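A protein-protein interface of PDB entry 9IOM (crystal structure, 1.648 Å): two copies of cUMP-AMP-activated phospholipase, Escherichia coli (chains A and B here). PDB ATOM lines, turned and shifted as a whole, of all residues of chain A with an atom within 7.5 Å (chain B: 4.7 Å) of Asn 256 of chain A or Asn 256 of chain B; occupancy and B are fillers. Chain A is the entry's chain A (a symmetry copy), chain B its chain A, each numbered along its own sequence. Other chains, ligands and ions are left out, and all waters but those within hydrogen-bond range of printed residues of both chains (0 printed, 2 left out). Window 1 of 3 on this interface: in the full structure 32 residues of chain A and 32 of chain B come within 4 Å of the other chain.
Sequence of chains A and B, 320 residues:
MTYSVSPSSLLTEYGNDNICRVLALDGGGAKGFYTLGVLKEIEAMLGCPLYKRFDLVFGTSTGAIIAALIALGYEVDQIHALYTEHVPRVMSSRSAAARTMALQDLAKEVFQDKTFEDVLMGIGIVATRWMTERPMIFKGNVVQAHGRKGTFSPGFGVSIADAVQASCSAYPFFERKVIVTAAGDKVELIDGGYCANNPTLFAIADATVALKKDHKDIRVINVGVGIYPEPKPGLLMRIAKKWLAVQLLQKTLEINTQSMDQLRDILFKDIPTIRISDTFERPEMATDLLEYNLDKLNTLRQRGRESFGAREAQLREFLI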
ATOM      1  N   GLU A 133     -10.256 -14.259 -35.156  1.00  0.00           N
ATOM      2  CA  GLU A 133     -10.792 -13.477 -34.030  1.00  0.00           C
ATOM      3  C   GLU A 133     -11.218 -14.368 -32.866  1.00  0.00           C
ATOM      4  O   GLU A 133     -12.114 -14.014 -32.092  1.00  0.00           O
ATOM      5  CB  GLU A 133     -11.946 -12.576 -34.490  1.00  0.00           C
ATOM      6  CG  GLU A 133     -11.424 -11.516 -35.477  1.00  0.00           C
ATOM      7  CD  GLU A 133     -12.492 -10.630 -36.080  1.00  0.00           C
ATOM      8  OE1 GLU A 133     -13.593 -11.115 -36.388  1.00  0.00           O
ATOM      9  OE2 GLU A 133     -12.206  -9.425 -36.248  1.00  0.00           O
ATOM     10  N   GLY A 193      -6.006 -10.633 -23.998  1.00  0.00           N
ATOM     11  CA  GLY A 193      -7.020  -9.920 -23.237  1.00  0.00           C
ATOM     12  C   GLY A 193      -8.239  -9.545 -24.046  1.00  0.00           C
ATOM     13  O   GLY A 193      -9.299  -9.277 -23.470  1.00  0.00           O
ATOM     14  N   TYR A 194      -8.121  -9.522 -25.381  1.00  0.00           N
ATOM     15  CA  TYR A 194      -9.270  -9.228 -26.226  1.00  0.00           C
ATOM     16  C   TYR A 194     -10.309 -10.339 -26.201  1.00  0.00           C
ATOM     17  O   TYR A 194     -11.485 -10.080 -26.460  1.00  0.00           O
ATOM     18  CB  TYR A 194      -8.810  -8.977 -27.668  1.00  0.00           C
ATOM     19  CG  TYR A 194      -8.084  -7.675 -27.849  1.00  0.00           C
ATOM     20  CD1 TYR A 194      -8.741  -6.472 -27.651  1.00  0.00           C
ATOM     21  CD2 TYR A 194      -6.750  -7.637 -28.229  1.00  0.00           C
ATOM     22  CE1 TYR A 194      -8.089  -5.261 -27.816  1.00  0.00           C
ATOM     23  CE2 TYR A 194      -6.093  -6.432 -28.409  1.00  0.00           C
ATOM     24  CZ  TYR A 194      -6.772  -5.244 -28.195  1.00  0.00           C
ATOM     25  OH  TYR A 194      -6.148  -4.028 -28.366  1.00  0.00           O
ATOM     26  N   CYS A 195      -9.914 -11.578 -25.913  1.00  0.00           N
ATOM     27  CA  CYS A 195     -10.889 -12.655 -25.832  1.00  0.00           C
ATOM     28  C   CYS A 195     -10.993 -13.275 -24.455  1.00  0.00           C
ATOM     29  O   CYS A 195     -12.012 -13.897 -24.151  1.00  0.00           O
ATOM     30  CB  CYS A 195     -10.578 -13.765 -26.856  1.00  0.00           C
ATOM     31  SG  CYS A 195      -8.990 -14.560 -26.651  1.00  0.00           S
ATOM     32  N   ALA A 196      -9.978 -13.133 -23.616  1.00  0.00           N
ATOM     33  CA  ALA A 196     -10.049 -13.794 -22.328  1.00  0.00           C
ATOM     34  C   ALA A 196      -9.072 -13.178 -21.346  1.00  0.00           C
ATOM     35  O   ALA A 196      -8.236 -13.886 -20.776  1.00  0.00           O
ATOM     36  CB  ALA A 196      -9.776 -15.290 -22.488  1.00  0.00           C
ATOM     37  N   ASN A 197      -9.195 -11.866 -21.106  1.00  0.00           N
ATOM     38  CA  ASN A 197      -8.312 -11.252 -20.125  1.00  0.00           C
ATOM     39  C   ASN A 197      -8.436 -11.939 -18.771  1.00  0.00           C
ATOM     40  O   ASN A 197      -7.449 -12.035 -18.026  1.00  0.00           O
ATOM     41  CB  ASN A 197      -8.600  -9.771 -19.963  1.00  0.00           C
ATOM     42  CG  ASN A 197      -7.519  -9.098 -19.182  1.00  0.00           C
ATOM     43  OD1 ASN A 197      -6.349  -9.150 -19.569  1.00  0.00           O
ATOM     44  ND2 ASN A 197      -7.871  -8.545 -18.030  1.00  0.00           N
ATOM     45  N   ASN A 198      -9.645 -12.388 -18.432  1.00  0.00           N
ATOM     46  CA  ASN A 198      -9.907 -13.296 -17.328  1.00  0.00           C
ATOM     47  C   ASN A 198      -9.971 -14.692 -17.922  1.00  0.00           C
ATOM     48  O   ASN A 198     -10.979 -15.036 -18.560  1.00  0.00           O
ATOM     49  CB  ASN A 198     -11.226 -12.919 -16.642  1.00  0.00           C
ATOM     50  CG  ASN A 198     -11.686 -13.935 -15.611  1.00  0.00           C
ATOM     51  OD1 ASN A 198     -11.081 -14.998 -15.426  1.00  0.00           O
ATOM     52  ND2 ASN A 198     -12.784 -13.601 -14.923  1.00  0.00           N
ATOM     53  N   LEU A 249      -9.966   1.116 -24.855  1.00  0.00           N
ATOM     54  CA  LEU A 249      -9.256  -0.142 -24.636  1.00  0.00           C
ATOM     55  C   LEU A 249      -9.372  -0.591 -23.186  1.00  0.00           C
ATOM     56  O   LEU A 249      -9.717  -1.742 -22.903  1.00  0.00           O
ATOM     57  CB  LEU A 249      -7.784   0.011 -25.036  1.00  0.00           C
ATOM     58  CG  LEU A 249      -6.916  -1.214 -24.729  1.00  0.00           C
ATOM     59  CD1 LEU A 249      -7.319  -2.412 -25.576  1.00  0.00           C
ATOM     60  CD2 LEU A 249      -5.431  -0.878 -24.929  1.00  0.00           C
ATOM     61  N   GLN A 250      -9.125   0.330 -22.244  1.00  0.00           N
ATOM     62  CA  GLN A 250      -9.155  -0.039 -20.833  1.00  0.00           C
ATOM     63  C   GLN A 250     -10.560  -0.445 -20.392  1.00  0.00           C
ATOM     64  O   GLN A 250     -10.737  -1.458 -19.699  1.00  0.00           O
ATOM     65  CB  GLN A 250      -8.646   1.131 -19.992  1.00  0.00           C
ATOM     66  CG  GLN A 250      -8.709   0.842 -18.504  1.00  0.00           C
ATOM     67  CD  GLN A 250      -7.690  -0.185 -18.087  1.00  0.00           C
ATOM     68  OE1 GLN A 250      -6.625  -0.305 -18.705  1.00  0.00           O
ATOM     69  NE2 GLN A 250      -7.997  -0.939 -17.021  1.00  0.00           N
ATOM     70  N   LYS A 251     -11.579   0.335 -20.780  1.00  0.00           N
ATOM     71  CA  LYS A 251     -12.929   0.015 -20.311  1.00  0.00           C
ATOM     72  C   LYS A 251     -13.424  -1.301 -20.897  1.00  0.00           C
ATOM     73  O   LYS A 251     -14.033  -2.113 -20.185  1.00  0.00           O
ATOM     74  CB  LYS A 251     -13.903   1.138 -20.649  1.00  0.00           C
ATOM     75  CG  LYS A 251     -15.255   0.991 -19.937  1.00  0.00           C
ATOM     76  CD  LYS A 251     -15.142   1.219 -18.421  1.00  0.00           C
ATOM     77  CE  LYS A 251     -16.508   1.080 -17.743  1.00  0.00           C
ATOM     78  NZ  LYS A 251     -16.433   1.294 -16.259  1.00  0.00           N
ATOM     79  N   THR A 252     -13.149  -1.553 -22.185  1.00  0.00           N
ATOM     80  CA  THR A 252     -13.591  -2.825 -22.755  1.00  0.00           C
ATOM     81  C   THR A 252     -12.874  -4.002 -22.095  1.00  0.00           C
ATOM     82  O   THR A 252     -13.490  -5.043 -21.851  1.00  0.00           O
ATOM     83  CB  THR A 252     -13.406  -2.828 -24.278  1.00  0.00           C
ATOM     84  OG1 THR A 252     -12.040  -2.589 -24.622  1.00  0.00           O
ATOM     85  CG2 THR A 252     -14.229  -1.740 -24.890  1.00  0.00           C
ATOM     86  N   LEU A 253     -11.588  -3.832 -21.764  1.00  0.00           N
ATOM     87  CA  LEU A 253     -10.831  -4.861 -21.066  1.00  0.00           C
ATOM     88  C   LEU A 253     -11.442  -5.159 -19.702  1.00  0.00           C
ATOM     89  O   LEU A 253     -11.583  -6.321 -19.312  1.00  0.00           O
ATOM     90  CB  LEU A 253      -9.385  -4.395 -20.904  1.00  0.00           C
ATOM     91  CG  LEU A 253      -8.393  -5.412 -20.379  1.00  0.00           C
ATOM     92  CD1 LEU A 253      -8.303  -6.542 -21.400  1.00  0.00           C
ATOM     93  CD2 LEU A 253      -7.043  -4.706 -20.170  1.00  0.00           C
ATOM     94  N   GLU A 254     -11.820  -4.111 -18.971  1.00  0.00           N
ATOM     95  CA  GLU A 254     -12.440  -4.316 -17.667  1.00  0.00           C
ATOM     96  C   GLU A 254     -13.776  -5.034 -17.793  1.00  0.00           C
ATOM     97  O   GLU A 254     -14.094  -5.924 -16.990  1.00  0.00           O
ATOM     98  CB  GLU A 254     -12.633  -2.966 -16.976  1.00  0.00           C
ATOM     99  CG  GLU A 254     -11.327  -2.303 -16.589  1.00  0.00           C
ATOM    100  CD  GLU A 254     -11.534  -0.900 -16.055  1.00  0.00           C
ATOM    101  OE1 GLU A 254     -10.519  -0.250 -15.704  1.00  0.00           O
ATOM    102  OE2 GLU A 254     -12.704  -0.436 -15.988  1.00  0.00           O
ATOM    103  N   ILE A 255     -14.587  -4.641 -18.776  1.00  0.00           N
ATOM    104  CA  ILE A 255     -15.877  -5.299 -18.954  1.00  0.00           C
ATOM    105  C   ILE A 255     -15.678  -6.771 -19.307  1.00  0.00           C
ATOM    106  O   ILE A 255     -16.338  -7.653 -18.749  1.00  0.00           O
ATOM    107  CB  ILE A 255     -16.709  -4.547 -20.004  1.00  0.00           C
ATOM    108  CG1 ILE A 255     -17.089  -3.157 -19.476  1.00  0.00           C
ATOM    109  CG2 ILE A 255     -17.985  -5.315 -20.336  1.00  0.00           C
ATOM    110  CD1 ILE A 255     -17.579  -2.232 -20.555  1.00  0.00           C
ATOM    111  N   ASN A 256     -14.727  -7.079 -20.194  1.00  0.00           N
ATOM    112  CA  ASN A 256     -14.530  -8.485 -20.521  1.00  0.00           C
ATOM    113  C   ASN A 256     -14.077  -9.270 -19.293  1.00  0.00           C
ATOM    114  O   ASN A 256     -14.516 -10.408 -19.076  1.00  0.00           O
ATOM    115  CB  ASN A 256     -13.563  -8.604 -21.693  1.00  0.00           C
ATOM    116  CG  ASN A 256     -14.267  -8.297 -23.037  1.00  0.00           C
ATOM    117  OD1 ASN A 256     -15.479  -8.550 -23.187  1.00  0.00           O
ATOM    118  ND2 ASN A 256     -13.525  -7.752 -24.000  1.00  0.00           N
ATOM    119  N   THR A 257     -13.264  -8.645 -18.438  1.00  0.00           N
ATOM    120  CA  THR A 257     -12.784  -9.305 -17.226  1.00  0.00           C
ATOM    121  C   THR A 257     -13.929  -9.594 -16.256  1.00  0.00           C
ATOM    122  O   THR A 257     -14.095 -10.731 -15.799  1.00  0.00           O
ATOM    123  CB  THR A 257     -11.715  -8.427 -16.575  1.00  0.00           C
ATOM    124  OG1 THR A 257     -10.669  -8.207 -17.542  1.00  0.00           O
ATOM    125  CG2 THR A 257     -11.147  -9.114 -15.349  1.00  0.00           C
ATOM    126  N   GLN A 258     -14.756  -8.589 -15.981  1.00  0.00           N
ATOM    127  CA  GLN A 258     -15.846  -8.759 -15.019  1.00  0.00           C
ATOM    128  C   GLN A 258     -16.967  -9.618 -15.590  1.00  0.00           C
ATOM    129  O   GLN A 258     -17.517 -10.473 -14.891  1.00  0.00           O
ATOM    130  CB  GLN A 258     -16.391  -7.398 -14.608  1.00  0.00           C
ATOM    131  CG  GLN A 258     -15.329  -6.496 -14.036  1.00  0.00           C
ATOM    132  CD  GLN A 258     -14.870  -6.985 -12.698  1.00  0.00           C
ATOM    133  OE1 GLN A 258     -15.684  -7.200 -11.783  1.00  0.00           O
ATOM    134  NE2 GLN A 258     -13.564  -7.197 -12.569  1.00  0.00           N
ATOM    135  N   SER A 259     -17.330  -9.394 -16.853  1.00  0.00           N
ATOM    136  CA  SER A 259     -18.426 -10.162 -17.441  1.00  0.00           C
ATOM    137  C   SER A 259     -18.068 -11.627 -17.600  1.00  0.00           C
ATOM    138  O   SER A 259     -18.948 -12.486 -17.481  1.00  0.00           O
ATOM    139  CB  SER A 259     -18.827  -9.564 -18.787  1.00  0.00           C
ATOM    140  OG  SER A 259     -19.421  -8.288 -18.599  1.00  0.00           O
ATOM    141  N   MET A 260     -16.797 -11.935 -17.902  1.00  0.00           N
ATOM    142  CA  MET A 260     -16.371 -13.329 -17.898  1.00  0.00           C
ATOM    143  C   MET A 260     -16.588 -13.966 -16.534  1.00  0.00           C
ATOM    144  O   MET A 260     -17.020 -15.117 -16.444  1.00  0.00           O
ATOM    145  CB  MET A 260     -14.911 -13.431 -18.317  1.00  0.00           C
ATOM    146  CG  MET A 260     -14.736 -13.532 -19.815  1.00  0.00           C
ATOM    147  SD  MET A 260     -14.891 -15.257 -20.344  1.00  0.00           S
ATOM    148  CE  MET A 260     -13.559 -15.304 -21.543  1.00  0.00           C
ATOM    149  N   ASP A 261     -16.305 -13.222 -15.460  1.00  0.00           N
ATOM    150  CA  ASP A 261     -16.563 -13.754 -14.128  1.00  0.00           C
ATOM    151  C   ASP A 261     -18.055 -14.004 -13.907  1.00  0.00           C
ATOM    152  O   ASP A 261     -18.436 -15.012 -13.306  1.00  0.00           O
ATOM    153  CB  ASP A 261     -16.018 -12.803 -13.068  1.00  0.00           C
ATOM    154  CG  ASP A 261     -16.211 -13.346 -11.669  1.00  0.00           C
ATOM    155  OD1 ASP A 261     -15.677 -14.435 -11.396  1.00  0.00           O
ATOM    156  OD2 ASP A 261     -16.915 -12.697 -10.875  1.00  0.00           O
ATOM    157  N   GLN A 262     -18.907 -13.094 -14.369  1.00  0.00           N
ATOM    158  CA  GLN A 262     -20.342 -13.284 -14.199  1.00  0.00           C
ATOM    159  C   GLN A 262     -20.835 -14.475 -15.005  1.00  0.00           C
ATOM    160  O   GLN A 262     -21.677 -15.250 -14.529  1.00  0.00           O
ATOM    161  CB  GLN A 262     -21.085 -12.024 -14.617  1.00  0.00           C
ATOM    162  CG  GLN A 262     -22.559 -12.060 -14.270  1.00  0.00           C
ATOM    163  CD  GLN A 262     -22.793 -12.014 -12.766  1.00  0.00           C
ATOM    164  OE1 GLN A 262     -21.936 -11.544 -12.002  1.00  0.00           O
ATOM    165  NE2 GLN A 262     -23.952 -12.505 -12.331  1.00  0.00           N
ATOM    166  N   GLY B 193     -23.271  -5.096 -26.398  1.00  0.00           N
ATOM    167  CA  GLY B 193     -22.217  -5.701 -27.198  1.00  0.00           C
ATOM    168  C   GLY B 193     -20.875  -5.742 -26.507  1.00  0.00           C
ATOM    169  O   GLY B 193     -20.007  -6.530 -26.899  1.00  0.00           O
ATOM    170  N   TYR B 194     -20.677  -4.911 -25.474  1.00  0.00           N
ATOM    171  CA  TYR B 194     -19.429  -4.938 -24.724  1.00  0.00           C
ATOM    172  C   TYR B 194     -19.271  -6.211 -23.905  1.00  0.00           C
ATOM    173  O   TYR B 194     -18.145  -6.603 -23.598  1.00  0.00           O
ATOM    174  CB  TYR B 194     -19.343  -3.713 -23.804  1.00  0.00           C
ATOM    175  CG  TYR B 194     -19.111  -2.425 -24.541  1.00  0.00           C
ATOM    176  CD1 TYR B 194     -17.933  -2.218 -25.238  1.00  0.00           C
ATOM    177  CD2 TYR B 194     -20.055  -1.408 -24.534  1.00  0.00           C
ATOM    178  CE1 TYR B 194     -17.699  -1.035 -25.921  1.00  0.00           C
ATOM    179  CE2 TYR B 194     -19.826  -0.218 -25.203  1.00  0.00           C
ATOM    180  CZ  TYR B 194     -18.642  -0.040 -25.899  1.00  0.00           C
ATOM    181  OH  TYR B 194     -18.383   1.132 -26.574  1.00  0.00           O
ATOM    182  N   THR B 252     -12.731  -4.993 -31.463  1.00  0.00           N
ATOM    183  CA  THR B 252     -13.012  -5.675 -30.201  1.00  0.00           C
ATOM    184  C   THR B 252     -14.401  -6.313 -30.218  1.00  0.00           C
ATOM    185  O   THR B 252     -14.579  -7.420 -29.702  1.00  0.00           O
ATOM    186  CB  THR B 252     -12.843  -4.714 -29.018  1.00  0.00           C
ATOM    187  OG1 THR B 252     -13.702  -3.581 -29.159  1.00  0.00           O
ATOM    188  CG2 THR B 252     -11.434  -4.217 -28.966  1.00  0.00           C
ATOM    189  N   LEU B 253     -15.377  -5.646 -30.845  1.00  0.00           N
ATOM    190  CA  LEU B 253     -16.718  -6.195 -30.985  1.00  0.00           C
ATOM    191  C   LEU B 253     -16.698  -7.493 -31.784  1.00  0.00           C
ATOM    192  O   LEU B 253     -17.349  -8.473 -31.415  1.00  0.00           O
ATOM    193  CB  LEU B 253     -17.611  -5.167 -31.676  1.00  0.00           C
ATOM    194  CG  LEU B 253     -19.093  -5.474 -31.732  1.00  0.00           C
ATOM    195  CD1 LEU B 253     -19.614  -5.509 -30.299  1.00  0.00           C
ATOM    196  CD2 LEU B 253     -19.780  -4.388 -32.576  1.00  0.00           C
ATOM    197  N   GLU B 254     -15.938  -7.512 -32.879  1.00  0.00           N
ATOM    198  CA  GLU B 254     -15.844  -8.727 -33.681  1.00  0.00           C
ATOM    199  C   GLU B 254     -15.192  -9.858 -32.899  1.00  0.00           C
ATOM    200  O   GLU B 254     -15.630 -11.016 -32.978  1.00  0.00           O
ATOM    201  CB  GLU B 254     -15.045  -8.438 -34.951  1.00  0.00           C
ATOM    202  CG  GLU B 254     -15.759  -7.503 -35.905  1.00  0.00           C
ATOM    203  CD  GLU B 254     -14.885  -7.103 -37.077  1.00  0.00           C
ATOM    204  OE1 GLU B 254     -15.373  -6.325 -37.934  1.00  0.00           O
ATOM    205  OE2 GLU B 254     -13.711  -7.556 -37.148  1.00  0.00           O
ATOM    206  N   ILE B 255     -14.123  -9.553 -32.164  1.00  0.00           N
ATOM    207  CA  ILE B 255     -13.461 -10.594 -31.385  1.00  0.00           C
ATOM    208  C   ILE B 255     -14.406 -11.140 -30.317  1.00  0.00           C
ATOM    209  O   ILE B 255     -14.522 -12.355 -30.132  1.00  0.00           O
ATOM    210  CB  ILE B 255     -12.151 -10.053 -30.793  1.00  0.00           C
ATOM    211  CG1 ILE B 255     -11.148  -9.759 -31.916  1.00  0.00           C
ATOM    212  CG2 ILE B 255     -11.533 -11.063 -29.830  1.00  0.00           C
ATOM    213  CD1 ILE B 255      -9.998  -8.900 -31.469  1.00  0.00           C
ATOM    214  N   ASN B 256     -15.148 -10.264 -29.631  1.00  0.00           N
ATOM    215  CA  ASN B 256     -16.058 -10.788 -28.621  1.00  0.00           C
ATOM    216  C   ASN B 256     -17.128 -11.670 -29.259  1.00  0.00           C
ATOM    217  O   ASN B 256     -17.495 -12.714 -28.703  1.00  0.00           O
ATOM    218  CB  ASN B 256     -16.642  -9.633 -27.815  1.00  0.00           C
ATOM    219  CG  ASN B 256     -15.632  -9.112 -26.765  1.00  0.00           C
ATOM    220  OD1 ASN B 256     -14.800  -9.886 -26.251  1.00  0.00           O
ATOM    221  ND2 ASN B 256     -15.693  -7.818 -26.452  1.00  0.00           N
ATOM    222  N   THR B 257     -17.575 -11.308 -30.463  1.00  0.00           N
ATOM    223  CA  THR B 257     -18.589 -12.092 -31.164  1.00  0.00           C
ATOM    224  C   THR B 257     -18.064 -13.476 -31.541  1.00  0.00           C
ATOM    225  O   THR B 257     -18.695 -14.495 -31.235  1.00  0.00           O
ATOM    226  CB  THR B 257     -19.048 -11.318 -32.400  1.00  0.00           C
ATOM    227  OG1 THR B 257     -19.537 -10.034 -31.965  1.00  0.00           O
ATOM    228  CG2 THR B 257     -20.150 -12.074 -33.114  1.00  0.00           C
ATOM    229  N   GLN B 258     -16.884 -13.528 -32.154  1.00  0.00           N
ATOM    230  CA  GLN B 258     -16.330 -14.806 -32.603  1.00  0.00           C
ATOM    231  C   GLN B 258     -15.836 -15.644 -31.431  1.00  0.00           C
ATOM    232  O   GLN B 258     -16.052 -16.859 -31.397  1.00  0.00           O
ATOM    233  CB  GLN B 258     -15.190 -14.560 -33.583  1.00  0.00           C
ATOM    234  CG  GLN B 258     -15.612 -13.731 -34.768  1.00  0.00           C
ATOM    235  CD  GLN B 258     -16.535 -14.499 -35.661  1.00  0.00           C
ATOM    236  OE1 GLN B 258     -16.214 -15.615 -36.104  1.00  0.00           O
ATOM    237  NE2 GLN B 258     -17.710 -13.930 -35.917  1.00  0.00           N
ATOM    238  N   SER B 259     -15.159 -15.018 -30.469  1.00  0.00           N
ATOM    239  CA  SER B 259     -14.628 -15.780 -29.340  1.00  0.00           C
ATOM    240  C   SER B 259     -15.734 -16.337 -28.464  1.00  0.00           C
ATOM    241  O   SER B 259     -15.574 -17.422 -27.895  1.00  0.00           O
ATOM    242  CB  SER B 259     -13.685 -14.910 -28.513  1.00  0.00           C
ATOM    243  OG  SER B 259     -12.510 -14.617 -29.256  1.00  0.00           O
ATOM    244  N   MET B 260     -16.847 -15.602 -28.314  1.00  0.00           N
ATOM    245  CA  MET B 260     -17.999 -16.170 -27.623  1.00  0.00           C
ATOM    246  C   MET B 260     -18.486 -17.434 -28.314  1.00  0.00           C
ATOM    247  O   MET B 260     -18.841 -18.412 -27.650  1.00  0.00           O
ATOM    248  CB  MET B 260     -19.116 -15.138 -27.533  1.00  0.00           C
ATOM    249  CG  MET B 260     -19.001 -14.254 -26.312  1.00  0.00           C
ATOM    250  SD  MET B 260     -19.780 -15.057 -24.888  1.00  0.00           S
ATOM    251  CE  MET B 260     -20.603 -13.632 -24.177  1.00  0.00           C
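Tyr 194 of chain A touches Thr 252 of chain B, and with the chains exchanged Thr 252 of chain A touches Tyr 194 of chain B. Tyr 194 of chain A touches Ile 255 of chain B, and with the chains exchanged Ile 255 of chain A touches Tyr 194 of chain B. Tyr 194 of chain A touches Asn 256 of chain B, and with the chains exchanged Asn 256 of chain A touches Tyr 194 of chain B. Asn 256 of chain B touches its own counterpart, Asn 256 of chain A. Positions printed for both chains: 193, 194, 252, 253, 254, 255, 256, 257, 258, 259 and 260. Of the 12 pairs that touch across the chains among the printed residues, 7 have their exchanged pair printed and touching as well.
Among the printed residues, pairs that only touch across the chains: Cys 195 of chain A with Ser 259 of chain B (3.2 Å), Glu 133 of chain A with Gln 258 of chain B (3.5 Å), Ile 255 of chain A with Tyr 194 of chain B (3.5 Å), Tyr 194 of chain A with Ile 255 of chain B (3.5 Å), Glu 133 of chain A with Ile 255 of chain B (3.5 Å), Thr 252 of chain A with Tyr 194 of chain B (3.7 Å) and Tyr 194 of chain A with Thr 252 of chain B (3.7 Å).
O of Tyr 194 of chain B sits close to OD1 of Asn 256 of chain A. The side-chain carboxylate of Glu 133 of chain A lies close to the side-chain carboxylate of Glu 254 of chain B (2.6 Å). OD1 of Asn 256 of chain B sits close to O of Tyr 194 of chain A, 3.3 Å away. ND2 of Asn 256 of chain A lies close to ND2 of Asn 256 of chain B (3.3 Å). The backbone carbonyl oxygen (O) of Glu 133 of chain A lies within hydrogen-bond range of the side-chain hydroxyl (OG) of Ser 259 of chain B (2.9 Å).
Of chain B, only Tyr 194 and Asn 256 come within 4 Å of Asn 256 of chain A. Asn 256 of chain B touches just these residues of chain A: Tyr 194 (3.3 Å) and Asn 256 (3.3 Å). Of the printed residues of chain A, Glu 254 of chain B touches Glu 133. Printed residues of chain B within 4 Å of Cys 195 of chain A: Ser 259. Printed residues of chain A within 4 Å of Gln 258 of chain B: Glu 133. Of the printed residues of chain A, Tyr 194 of chain B touches Thr 252 (3.7 Å), Ile 255 (3.5 Å) and Asn 256 (3.3 Å). Printed residues of chain B within 4 Å of Ile 255 of chain A: Tyr 194. The nearest printed residue of chain B that does not touch Asn 256 of chain A is Thr 252 of chain B (5.8 Å).
Printed residues of chain B that touch a printed residue of chain A: Tyr 194, Thr 252, Glu 254, Ile 255, Asn 256, Gln 258 and Ser 259. Hydrophobic or aromatic side chains of chain B that line the printed part of chain A: Tyr 194 and Ile 255. Printed residues of chain A that touch a printed residue of chain B: Glu 133, Tyr 194, Cys 195, Thr 252, Ile 255 and Asn 256. Hydrophobic or aromatic side chains of chain A that line the printed part of chain B: Tyr 194 and Ile 255. Among the printed residues, no Asp or Glu carboxylate lies within 4 Å of a Lys or Arg side-chain nitrogen of the other chain.
The side-chain amide nitrogen of Asn 256 of chain B lies within hydrogen-bond range of the backbone carbonyl oxygen of Thr 252 of chain B (3.5 Å). OG of Ser 259 of chain B sits close to O of Ile 255 of chain B, at 3.2 Å. The side-chain hydroxyl (OG1) of Thr 252 of chain A sits at hydrogen-bond distance from the backbone carbonyl oxygen (O) of Leu 249 of chain A, 3.0 Å away. The side-chain amide nitrogen of Asn 256 of chain A is in hydrogen-bond range of the backbone carbonyl oxygen of Thr 252 of chain A, 3.5 Å away. The backbone carbonyl oxygen of Ile 255 of chain A lies close to the side-chain hydroxyl of Ser 259 of chain A, 3.2 Å away.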
